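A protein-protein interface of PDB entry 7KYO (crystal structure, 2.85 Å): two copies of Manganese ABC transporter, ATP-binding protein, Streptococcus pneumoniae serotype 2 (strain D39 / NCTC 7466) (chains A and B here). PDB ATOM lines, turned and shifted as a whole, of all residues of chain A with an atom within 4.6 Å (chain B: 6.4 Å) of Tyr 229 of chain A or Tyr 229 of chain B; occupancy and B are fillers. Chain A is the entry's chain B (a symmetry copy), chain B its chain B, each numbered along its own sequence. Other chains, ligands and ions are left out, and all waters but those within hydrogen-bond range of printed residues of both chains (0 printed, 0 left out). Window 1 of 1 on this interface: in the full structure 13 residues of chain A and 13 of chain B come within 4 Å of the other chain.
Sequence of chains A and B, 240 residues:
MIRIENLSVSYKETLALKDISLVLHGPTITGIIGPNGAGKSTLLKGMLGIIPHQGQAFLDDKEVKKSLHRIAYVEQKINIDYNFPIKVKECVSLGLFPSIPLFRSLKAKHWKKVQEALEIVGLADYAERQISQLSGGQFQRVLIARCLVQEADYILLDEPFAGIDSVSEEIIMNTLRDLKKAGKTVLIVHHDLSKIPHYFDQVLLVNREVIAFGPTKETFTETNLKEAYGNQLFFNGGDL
Of chain B, only Asp 192, Leu 193 and Tyr 229 come within 4 Å of Tyr 229 of chain A.
Of chain A, only Asp 192, Leu 193 and Tyr 229 come within 4 Å of Tyr 229 of chain B.
Of the printed residues of chain A, Asp 192 of chain B touches Tyr 229 (3.5 Å) and Asn 231 (3.4 Å).
Of the printed residues of chain A, Asn 231 of chain B touches Asp 192.
The nearest residue of chain B that does not touch Tyr 229 of chain A is Ser 194 of chain B (4.7 Å).
The nearest printed residue of chain A that does not touch Tyr 229 of chain B is Pro 35 of chain A (6.4 Å).
Of the 12 printed residues of chain A, 5 touch a printed residue of chain B.
Among the printed residues, merely in contact across the chains: Asp 192 of chain A with Tyr 229 of chain B, Asp 192 of chain A with Asn 231 of chain B, Leu 193 of chain A with Gly 230 of chain B, Leu 193 of chain A with Phe 234 of chain B, Tyr 229 of chain A with Asp 192 of chain B, Tyr 229 of chain A with Tyr 229 of chain B, Gly 230 of chain A with Leu 193 of chain B, Gly 230 of chain A with Ser 194 of chain B and Asn 231 of chain A with Asp 192 of chain B.
N of Leu 193 of chain A lies within hydrogen-bond range of O of Tyr 229 of chain B (2.9 Å).
N of Leu 193 of chain B sits at hydrogen-bond distance from O of Tyr 229 of chain A, at 2.9 Å.
The side-chain carboxylate (OD2) of Asp 192 of chain B sits at hydrogen-bond distance from a ring nitrogen (NE2) of His 191 of chain B, at 3.3 Å.
The side-chain hydroxyl (OH) of Tyr 229 of chain A lies within hydrogen-bond range of the backbone carbonyl oxygen (O) of Gly 34 of chain A (3.0 Å).
The backbone carbonyl oxygen of Gly 34 of chain B is in hydrogen-bond range of the side-chain hydroxyl of Tyr 229 of chain B, at 3.0 Å.
The side-chain amide nitrogen (ND2) of Asn 207 of chain B is in hydrogen-bond range of the side-chain amide oxygen (OD1) of Asn 231 of chain B, 2.8 Å away.
The side-chain carboxylate (OD1) of Asp 192 of chain B is in hydrogen-bond range of the side-chain hydroxyl (OG) of Ser 194 of chain B (2.6 Å).
Asp 192 of chain A touches Tyr 229 of chain B, and with the chains exchanged Tyr 229 of chain A touches Asp 192 of chain B.
Asp 192 of chain A touches Asn 231 of chain B, and with the chains exchanged Asn 231 of chain A touches Asp 192 of chain B.
Leu 193 of chain A touches Gly 230 of chain B, and with the chains exchanged Gly 230 of chain A touches Leu 193 of chain B.
Tyr 229 of chain A touches its own counterpart, Tyr 229 of chain B.
Positions printed for both chains: 34, 35, 192, 193, 205, 225, 226, 227, 228, 229, 230 and 231.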
ATOM      1  N   GLY A  34       7.539  16.079   9.191  1.00  0.00           N
ATOM      2  CA  GLY A  34       7.508  16.994   8.051  1.00  0.00           C
ATOM      3  C   GLY A  34       7.705  18.431   8.485  1.00  0.00           C
ATOM      4  O   GLY A  34       7.872  18.695   9.674  1.00  0.00           O
ATOM      5  N   PRO A  35       7.693  19.375   7.524  1.00  0.00           N
ATOM      6  CA  PRO A  35       7.869  20.789   7.864  1.00  0.00           C
ATOM      7  C   PRO A  35       6.789  21.310   8.814  1.00  0.00           C
ATOM      8  O   PRO A  35       5.641  20.865   8.752  1.00  0.00           O
ATOM      9  CB  PRO A  35       7.771  21.493   6.507  1.00  0.00           C
ATOM     10  CG  PRO A  35       8.149  20.457   5.517  1.00  0.00           C
ATOM     11  CD  PRO A  35       7.608  19.175   6.066  1.00  0.00           C
ATOM     12  N   ASP A 192      10.121  17.849  15.418  1.00  0.00           N
ATOM     13  CA  ASP A 192      11.333  17.998  14.598  1.00  0.00           C
ATOM     14  C   ASP A 192      11.777  16.619  14.068  1.00  0.00           C
ATOM     15  O   ASP A 192      10.923  15.751  13.889  1.00  0.00           O
ATOM     16  CB  ASP A 192      12.422  18.762  15.380  1.00  0.00           C
ATOM     17  CG  ASP A 192      12.862  18.053  16.650  1.00  0.00           C
ATOM     18  OD1 ASP A 192      12.351  16.957  16.951  1.00  0.00           O
ATOM     19  OD2 ASP A 192      13.724  18.610  17.365  1.00  0.00           O
ATOM     20  N   LEU A 193      13.067  16.421  13.783  1.00  0.00           N
ATOM     21  CA  LEU A 193      13.571  15.118  13.326  1.00  0.00           C
ATOM     22  C   LEU A 193      14.530  14.485  14.346  1.00  0.00           C
ATOM     23  O   LEU A 193      15.555  13.906  13.975  1.00  0.00           O
ATOM     24  CB  LEU A 193      14.237  15.268  11.953  1.00  0.00           C
ATOM     25  CG  LEU A 193      13.352  15.827  10.835  1.00  0.00           C
ATOM     26  CD1 LEU A 193      14.159  15.991   9.556  1.00  0.00           C
ATOM     27  CD2 LEU A 193      12.139  14.939  10.593  1.00  0.00           C
ATOM     28  N   LEU A 205       5.505  10.890   6.429  1.00  0.00           N
ATOM     29  CA  LEU A 205       6.008  12.200   5.988  1.00  0.00           C
ATOM     30  C   LEU A 205       4.908  13.006   5.304  1.00  0.00           C
ATOM     31  O   LEU A 205       4.250  12.504   4.393  1.00  0.00           O
ATOM     32  CB  LEU A 205       7.216  12.051   5.054  1.00  0.00           C
ATOM     33  CG  LEU A 205       8.573  11.990   5.765  1.00  0.00           C
ATOM     34  CD1 LEU A 205       9.623  11.242   4.951  1.00  0.00           C
ATOM     35  CD2 LEU A 205       9.055  13.400   6.096  1.00  0.00           C
ATOM     36  N   LEU A 225      13.009  12.568   2.895  1.00  0.00           N
ATOM     37  CA  LEU A 225      13.148  13.826   3.646  1.00  0.00           C
ATOM     38  C   LEU A 225      13.413  15.031   2.736  1.00  0.00           C
ATOM     39  O   LEU A 225      12.881  16.116   2.977  1.00  0.00           O
ATOM     40  CB  LEU A 225      14.266  13.724   4.691  1.00  0.00           C
ATOM     41  CG  LEU A 225      14.041  12.794   5.885  1.00  0.00           C
ATOM     42  CD1 LEU A 225      15.326  12.669   6.688  1.00  0.00           C
ATOM     43  CD2 LEU A 225      12.904  13.282   6.770  1.00  0.00           C
ATOM     44  N   LYS A 226      14.230  14.828   1.700  1.00  0.00           N
ATOM     45  CA  LYS A 226      14.563  15.891   0.743  1.00  0.00           C
ATOM     46  C   LYS A 226      13.343  16.470   0.024  1.00  0.00           C
ATOM     47  O   LYS A 226      13.204  17.691  -0.049  1.00  0.00           O
ATOM     48  CB  LYS A 226      15.610  15.418  -0.280  1.00  0.00           C
ATOM     49  CG  LYS A 226      17.042  15.553   0.216  1.00  0.00           C
ATOM     50  CD  LYS A 226      18.056  14.981  -0.763  1.00  0.00           C
ATOM     51  CE  LYS A 226      19.470  15.104  -0.210  1.00  0.00           C
ATOM     52  NZ  LYS A 226      20.522  14.745  -1.205  1.00  0.00           N
ATOM     53  N   GLU A 227      12.465  15.614  -0.495  1.00  0.00           N
ATOM     54  CA  GLU A 227      11.265  16.099  -1.199  1.00  0.00           C
ATOM     55  C   GLU A 227      10.148  16.588  -0.262  1.00  0.00           C
ATOM     56  O   GLU A 227       9.270  17.337  -0.701  1.00  0.00           O
ATOM     57  CB  GLU A 227      10.741  15.077  -2.223  1.00  0.00           C
ATOM     58  CG  GLU A 227      10.086  13.816  -1.674  1.00  0.00           C
ATOM     59  CD  GLU A 227       9.502  12.931  -2.772  1.00  0.00           C
ATOM     60  OE1 GLU A 227       9.799  13.170  -3.966  1.00  0.00           O
ATOM     61  OE2 GLU A 227       8.743  11.986  -2.446  1.00  0.00           O
ATOM     62  N   ALA A 228      10.178  16.179   1.009  1.00  0.00           N
ATOM     63  CA  ALA A 228       9.252  16.711   2.015  1.00  0.00           C
ATOM     64  C   ALA A 228       9.643  18.130   2.423  1.00  0.00           C
ATOM     65  O   ALA A 228       8.835  19.051   2.326  1.00  0.00           O
ATOM     66  CB  ALA A 228       9.212  15.809   3.238  1.00  0.00           C
ATOM     67  N   TYR A 229      10.883  18.296   2.880  1.00  0.00           N
ATOM     68  CA  TYR A 229      11.387  19.600   3.334  1.00  0.00           C
ATOM     69  C   TYR A 229      11.794  20.533   2.195  1.00  0.00           C
ATOM     70  O   TYR A 229      11.892  21.743   2.399  1.00  0.00           O
ATOM     71  CB  TYR A 229      12.540  19.418   4.330  1.00  0.00           C
ATOM     72  CG  TYR A 229      12.061  18.938   5.681  1.00  0.00           C
ATOM     73  CD1 TYR A 229      11.853  17.581   5.933  1.00  0.00           C
ATOM     74  CD2 TYR A 229      11.786  19.845   6.705  1.00  0.00           C
ATOM     75  CE1 TYR A 229      11.400  17.141   7.168  1.00  0.00           C
ATOM     76  CE2 TYR A 229      11.333  19.414   7.943  1.00  0.00           C
ATOM     77  CZ  TYR A 229      11.141  18.062   8.170  1.00  0.00           C
ATOM     78  OH  TYR A 229      10.692  17.635   9.395  1.00  0.00           O
ATOM     79  N   GLY A 230      12.029  19.974   1.006  1.00  0.00           N
ATOM     80  CA  GLY A 230      12.301  20.761  -0.198  1.00  0.00           C
ATOM     81  C   GLY A 230      11.085  21.051  -1.065  1.00  0.00           C
ATOM     82  O   GLY A 230      11.220  21.705  -2.103  1.00  0.00           O
ATOM     83  N   ASN A 231       9.910  20.559  -0.657  1.00  0.00           N
ATOM     84  CA  ASN A 231       8.646  20.753  -1.388  1.00  0.00           C
ATOM     85  C   ASN A 231       8.730  20.282  -2.854  1.00  0.00           C
ATOM     86  O   ASN A 231       8.245  20.950  -3.777  1.00  0.00           O
ATOM     87  CB  ASN A 231       8.194  22.221  -1.270  1.00  0.00           C
ATOM     88  CG  ASN A 231       6.687  22.391  -1.392  1.00  0.00           C
ATOM     89  OD1 ASN A 231       5.912  21.597  -0.858  1.00  0.00           O
ATOM     90  ND2 ASN A 231       6.266  23.445  -2.082  1.00  0.00           N
ATOM     91  N   ILE B  33      18.490  29.428   6.298  1.00  0.00           N
ATOM     92  CA  ILE B  33      17.618  28.248   6.312  1.00  0.00           C
ATOM     93  C   ILE B  33      17.620  27.558   7.674  1.00  0.00           C
ATOM     94  O   ILE B  33      18.467  27.832   8.524  1.00  0.00           O
ATOM     95  CB  ILE B  33      17.989  27.248   5.192  1.00  0.00           C
ATOM     96  CG1 ILE B  33      19.435  26.756   5.326  1.00  0.00           C
ATOM     97  CG2 ILE B  33      17.785  27.896   3.827  1.00  0.00           C
ATOM     98  CD1 ILE B  33      19.719  25.510   4.514  1.00  0.00           C
ATOM     99  N   GLY B  34      16.652  26.668   7.867  1.00  0.00           N
ATOM    100  CA  GLY B  34      16.484  25.940   9.122  1.00  0.00           C
ATOM    101  C   GLY B  34      15.023  25.683   9.426  1.00  0.00           C
ATOM    102  O   GLY B  34      14.157  26.071   8.645  1.00  0.00           O
ATOM    103  N   PRO B  35      14.735  25.019  10.562  1.00  0.00           N
ATOM    104  CA  PRO B  35      13.345  24.738  10.931  1.00  0.00           C
ATOM    105  C   PRO B  35      12.507  26.007  11.099  1.00  0.00           C
ATOM    106  O   PRO B  35      13.026  27.040  11.529  1.00  0.00           O
ATOM    107  CB  PRO B  35      13.476  24.003  12.268  1.00  0.00           C
ATOM    108  CG  PRO B  35      14.837  23.416  12.244  1.00  0.00           C
ATOM    109  CD  PRO B  35      15.681  24.415  11.518  1.00  0.00           C
ATOM    110  N   ASN B  36      11.228  25.920  10.742  1.00  0.00           N
ATOM    111  CA  ASN B  36      10.295  27.024  10.932  1.00  0.00           C
ATOM    112  C   ASN B  36      10.109  27.297  12.428  1.00  0.00           C
ATOM    113  O   ASN B  36      10.059  26.368  13.237  1.00  0.00           O
ATOM    114  CB  ASN B  36       8.948  26.700  10.280  1.00  0.00           C
ATOM    115  CG  ASN B  36       7.973  27.858  10.341  1.00  0.00           C
ATOM    116  OD1 ASN B  36       6.905  27.752  10.945  1.00  0.00           O
ATOM    117  ND2 ASN B  36       8.337  28.974   9.719  1.00  0.00           N
ATOM    118  N   LYS B  40      15.429  31.810  12.601  1.00  0.00           N
ATOM    119  CA  LYS B  40      15.896  32.391  11.328  1.00  0.00           C
ATOM    120  C   LYS B  40      15.229  33.732  11.004  1.00  0.00           C
ATOM    121  O   LYS B  40      15.900  34.661  10.549  1.00  0.00           O
ATOM    122  CB  LYS B  40      15.739  31.414  10.154  1.00  0.00           C
ATOM    123  CG  LYS B  40      14.318  31.006   9.804  1.00  0.00           C
ATOM    124  CD  LYS B  40      14.326  29.971   8.695  1.00  0.00           C
ATOM    125  CE  LYS B  40      12.925  29.462   8.408  1.00  0.00           C
ATOM    126  NZ  LYS B  40      12.932  28.395   7.373  1.00  0.00           N
ATOM    127  N   HIS B 191      11.863  29.987   3.198  1.00  0.00           N
ATOM    128  CA  HIS B 191      10.732  29.328   3.875  1.00  0.00           C
ATOM    129  C   HIS B 191      10.795  27.788   3.913  1.00  0.00           C
ATOM    130  O   HIS B 191      10.067  27.166   4.688  1.00  0.00           O
ATOM    131  CB  HIS B 191       9.404  29.771   3.241  1.00  0.00           C
ATOM    132  CG  HIS B 191       9.173  29.214   1.870  1.00  0.00           C
ATOM    133  ND1 HIS B 191       9.644  29.825   0.728  1.00  0.00           N
ATOM    134  CD2 HIS B 191       8.537  28.091   1.462  1.00  0.00           C
ATOM    135  CE1 HIS B 191       9.302  29.106  -0.325  1.00  0.00           C
ATOM    136  NE2 HIS B 191       8.630  28.048   0.092  1.00  0.00           N
ATOM    137  N   ASP B 192      11.625  27.181   3.065  1.00  0.00           N
ATOM    138  CA  ASP B 192      11.816  25.723   3.067  1.00  0.00           C
ATOM    139  C   ASP B 192      13.217  25.379   2.521  1.00  0.00           C
ATOM    140  O   ASP B 192      14.126  26.195   2.667  1.00  0.00           O
ATOM    141  CB  ASP B 192      10.654  25.026   2.328  1.00  0.00           C
ATOM    142  CG  ASP B 192      10.541  25.430   0.867  1.00  0.00           C
ATOM    143  OD1 ASP B 192      11.356  26.243   0.388  1.00  0.00           O
ATOM    144  OD2 ASP B 192       9.610  24.937   0.192  1.00  0.00           O
ATOM    145  N   LEU B 193      13.411  24.191   1.939  1.00  0.00           N
ATOM    146  CA  LEU B 193      14.704  23.817   1.348  1.00  0.00           C
ATOM    147  C   LEU B 193      14.608  23.644  -0.175  1.00  0.00           C
ATOM    148  O   LEU B 193      15.195  22.719  -0.744  1.00  0.00           O
ATOM    149  CB  LEU B 193      15.237  22.547   2.021  1.00  0.00           C
ATOM    150  CG  LEU B 193      15.441  22.625   3.537  1.00  0.00           C
ATOM    151  CD1 LEU B 193      15.900  21.280   4.078  1.00  0.00           C
ATOM    152  CD2 LEU B 193      16.434  23.719   3.908  1.00  0.00           C
ATOM    153  N   SER B 194      13.897  24.568  -0.825  1.00  0.00           N
ATOM    154  CA  SER B 194      13.660  24.517  -2.264  1.00  0.00           C
ATOM    155  C   SER B 194      14.616  25.441  -3.022  1.00  0.00           C
ATOM    156  O   SER B 194      14.723  26.626  -2.696  1.00  0.00           O
ATOM    157  CB  SER B 194      12.212  24.904  -2.573  1.00  0.00           C
ATOM    158  OG  SER B 194      11.937  26.232  -2.171  1.00  0.00           O
ATOM    159  N   LEU B 205      22.684  28.125   8.296  1.00  0.00           N
ATOM    160  CA  LEU B 205      21.763  27.206   8.981  1.00  0.00           C
ATOM    161  C   LEU B 205      21.549  27.626  10.432  1.00  0.00           C
ATOM    162  O   LEU B 205      22.516  27.840  11.162  1.00  0.00           O
ATOM    163  CB  LEU B 205      22.265  25.757   8.917  1.00  0.00           C
ATOM    164  CG  LEU B 205      21.812  24.975   7.678  1.00  0.00           C
ATOM    165  CD1 LEU B 205      22.773  23.847   7.320  1.00  0.00           C
ATOM    166  CD2 LEU B 205      20.401  24.433   7.890  1.00  0.00           C
ATOM    167  N   ASN B 207      19.150  26.700  13.958  1.00  0.00           N
ATOM    168  CA  ASN B 207      18.126  26.109  14.841  1.00  0.00           C
ATOM    169  C   ASN B 207      17.974  26.965  16.094  1.00  0.00           C
ATOM    170  O   ASN B 207      16.863  27.305  16.485  1.00  0.00           O
ATOM    171  CB  ASN B 207      18.465  24.668  15.234  1.00  0.00           C
ATOM    172  CG  ASN B 207      17.260  23.904  15.789  1.00  0.00           C
ATOM    173  OD1 ASN B 207      16.303  24.491  16.295  1.00  0.00           O
ATOM    174  ND2 ASN B 207      17.308  22.585  15.696  1.00  0.00           N
ATOM    175  N   ASN B 224      25.089  18.723   7.912  1.00  0.00           N
ATOM    176  CA  ASN B 224      24.652  19.972   8.551  1.00  0.00           C
ATOM    177  C   ASN B 224      23.133  20.086   8.663  1.00  0.00           C
ATOM    178  O   ASN B 224      22.626  20.531   9.690  1.00  0.00           O
ATOM    179  CB  ASN B 224      25.202  21.191   7.801  1.00  0.00           C
ATOM    180  CG  ASN B 224      26.707  21.332   7.932  1.00  0.00           C
ATOM    181  OD1 ASN B 224      27.288  21.027   8.970  1.00  0.00           O
ATOM    182  ND2 ASN B 224      27.343  21.817   6.876  1.00  0.00           N
ATOM    183  N   LEU B 225      22.414  19.695   7.610  1.00  0.00           N
ATOM    184  CA  LEU B 225      20.942  19.681   7.635  1.00  0.00           C
ATOM    185  C   LEU B 225      20.380  18.754   8.720  1.00  0.00           C
ATOM    186  O   LEU B 225      19.388  19.091   9.368  1.00  0.00           O
ATOM    187  CB  LEU B 225      20.369  19.273   6.272  1.00  0.00           C
ATOM    188  CG  LEU B 225      20.546  20.249   5.106  1.00  0.00           C
ATOM    189  CD1 LEU B 225      20.105  19.586   3.812  1.00  0.00           C
ATOM    190  CD2 LEU B 225      19.776  21.540   5.334  1.00  0.00           C
ATOM    191  N   LYS B 226      21.019  17.596   8.906  1.00  0.00           N
ATOM    192  CA  LYS B 226      20.595  16.619   9.916  1.00  0.00           C
ATOM    193  C   LYS B 226      20.602  17.172  11.343  1.00  0.00           C
ATOM    194  O   LYS B 226      19.623  16.995  12.067  1.00  0.00           O
ATOM    195  CB  LYS B 226      21.433  15.332   9.838  1.00  0.00           C
ATOM    196  CG  LYS B 226      20.921  14.339   8.807  1.00  0.00           C
ATOM    197  CD  LYS B 226      21.822  13.122   8.668  1.00  0.00           C
ATOM    198  CE  LYS B 226      21.292  12.174   7.600  1.00  0.00           C
ATOM    199  NZ  LYS B 226      22.019  10.873   7.556  1.00  0.00           N
ATOM    200  N   GLU B 227      21.683  17.839  11.743  1.00  0.00           N
ATOM    201  CA  GLU B 227      21.759  18.402  13.102  1.00  0.00           C
ATOM    202  C   GLU B 227      20.960  19.703  13.284  1.00  0.00           C
ATOM    203  O   GLU B 227      20.643  20.069  14.420  1.00  0.00           O
ATOM    204  CB  GLU B 227      23.213  18.556  13.584  1.00  0.00           C
ATOM    205  CG  GLU B 227      24.050  19.648  12.929  1.00  0.00           C
ATOM    206  CD  GLU B 227      25.433  19.788  13.561  1.00  0.00           C
ATOM    207  OE1 GLU B 227      25.832  18.898  14.348  1.00  0.00           O
ATOM    208  OE2 GLU B 227      26.131  20.789  13.271  1.00  0.00           O
ATOM    209  N   ALA B 228      20.631  20.391  12.187  1.00  0.00           N
ATOM    210  CA  ALA B 228      19.740  21.555  12.241  1.00  0.00           C
ATOM    211  C   ALA B 228      18.289  21.125  12.451  1.00  0.00           C
ATOM    212  O   ALA B 228      17.641  21.564  13.398  1.00  0.00           O
ATOM    213  CB  ALA B 228      19.861  22.382  10.971  1.00  0.00           C
ATOM    214  N   TYR B 229      17.790  20.268  11.562  1.00  0.00           N
ATOM    215  CA  TYR B 229      16.401  19.790  11.624  1.00  0.00           C
ATOM    216  C   TYR B 229      16.176  18.687  12.658  1.00  0.00           C
ATOM    217  O   TYR B 229      15.037  18.448  13.061  1.00  0.00           O
ATOM    218  CB  TYR B 229      15.919  19.345  10.237  1.00  0.00           C
ATOM    219  CG  TYR B 229      15.658  20.517   9.318  1.00  0.00           C
ATOM    220  CD1 TYR B 229      16.690  21.104   8.585  1.00  0.00           C
ATOM    221  CD2 TYR B 229      14.377  21.061   9.201  1.00  0.00           C
ATOM    222  CE1 TYR B 229      16.453  22.188   7.753  1.00  0.00           C
ATOM    223  CE2 TYR B 229      14.131  22.144   8.371  1.00  0.00           C
ATOM    224  CZ  TYR B 229      15.172  22.704   7.650  1.00  0.00           C
ATOM    225  OH  TYR B 229      14.929  23.778   6.829  1.00  0.00           O
ATOM    226  N   GLY B 230      17.252  18.022  13.081  1.00  0.00           N
ATOM    227  CA  GLY B 230      17.198  17.032  14.159  1.00  0.00           C
ATOM    228  C   GLY B 230      17.526  17.570  15.544  1.00  0.00           C
ATOM    229  O   GLY B 230      17.509  16.806  16.513  1.00  0.00           O
ATOM    230  N   ASN B 231      17.839  18.867  15.639  1.00  0.00           N
ATOM    231  CA  ASN B 231      18.181  19.534  16.907  1.00  0.00           C
ATOM    232  C   ASN B 231      19.345  18.840  17.646  1.00  0.00           C
ATOM    233  O   ASN B 231      19.314  18.654  18.870  1.00  0.00           O
ATOM    234  CB  ASN B 231      16.924  19.662  17.787  1.00  0.00           C
ATOM    235  CG  ASN B 231      16.989  20.837  18.750  1.00  0.00           C
ATOM    236  OD1 ASN B 231      17.452  21.923  18.397  1.00  0.00           O
ATOM    237  ND2 ASN B 231      16.503  20.630  19.969  1.00  0.00           N
ATOM    238  N   GLN B 232      20.363  18.467  16.865  1.00  0.00           N
ATOM    239  CA  GLN B 232      21.551  17.742  17.338  1.00  0.00           C
ATOM    240  C   GLN B 232      21.219  16.407  18.027  1.00  0.00           C
ATOM    241  O   GLN B 232      21.953  15.958  18.909  1.00  0.00           O
ATOM    242  CB  GLN B 232      22.409  18.648  18.241  1.00  0.00           C
ATOM    243  CG  GLN B 232      22.887  19.931  17.558  1.00  0.00           C
ATOM    244  CD  GLN B 232      23.244  21.034  18.542  1.00  0.00           C
ATOM    245  OE1 GLN B 232      23.811  20.777  19.607  1.00  0.00           O
ATOM    246  NE2 GLN B 232      22.911  22.273  18.186  1.00  0.00           N
ATOM    247  N   PHE B 234      19.701  13.610  15.894  1.00  0.00           N
ATOM    248  CA  PHE B 234      19.217  12.893  14.714  1.00  0.00           C
ATOM    249  C   PHE B 234      19.558  11.407  14.804  1.00  0.00           C
ATOM    250  O   PHE B 234      20.721  11.034  14.961  1.00  0.00           O
ATOM    251  CB  PHE B 234      19.823  13.503  13.445  1.00  0.00           C
ATOM    252  CG  PHE B 234      19.121  13.100  12.179  1.00  0.00           C
ATOM    253  CD1 PHE B 234      19.492  11.945  11.495  1.00  0.00           C
ATOM    254  CD2 PHE B 234      18.089  13.879  11.664  1.00  0.00           C
ATOM    255  CE1 PHE B 234      18.845  11.573  10.325  1.00  0.00           C
ATOM    256  CE2 PHE B 234      17.438  13.514  10.493  1.00  0.00           C
ATOM    257  CZ  PHE B 234      17.816  12.359   9.823  1.00  0.00           C
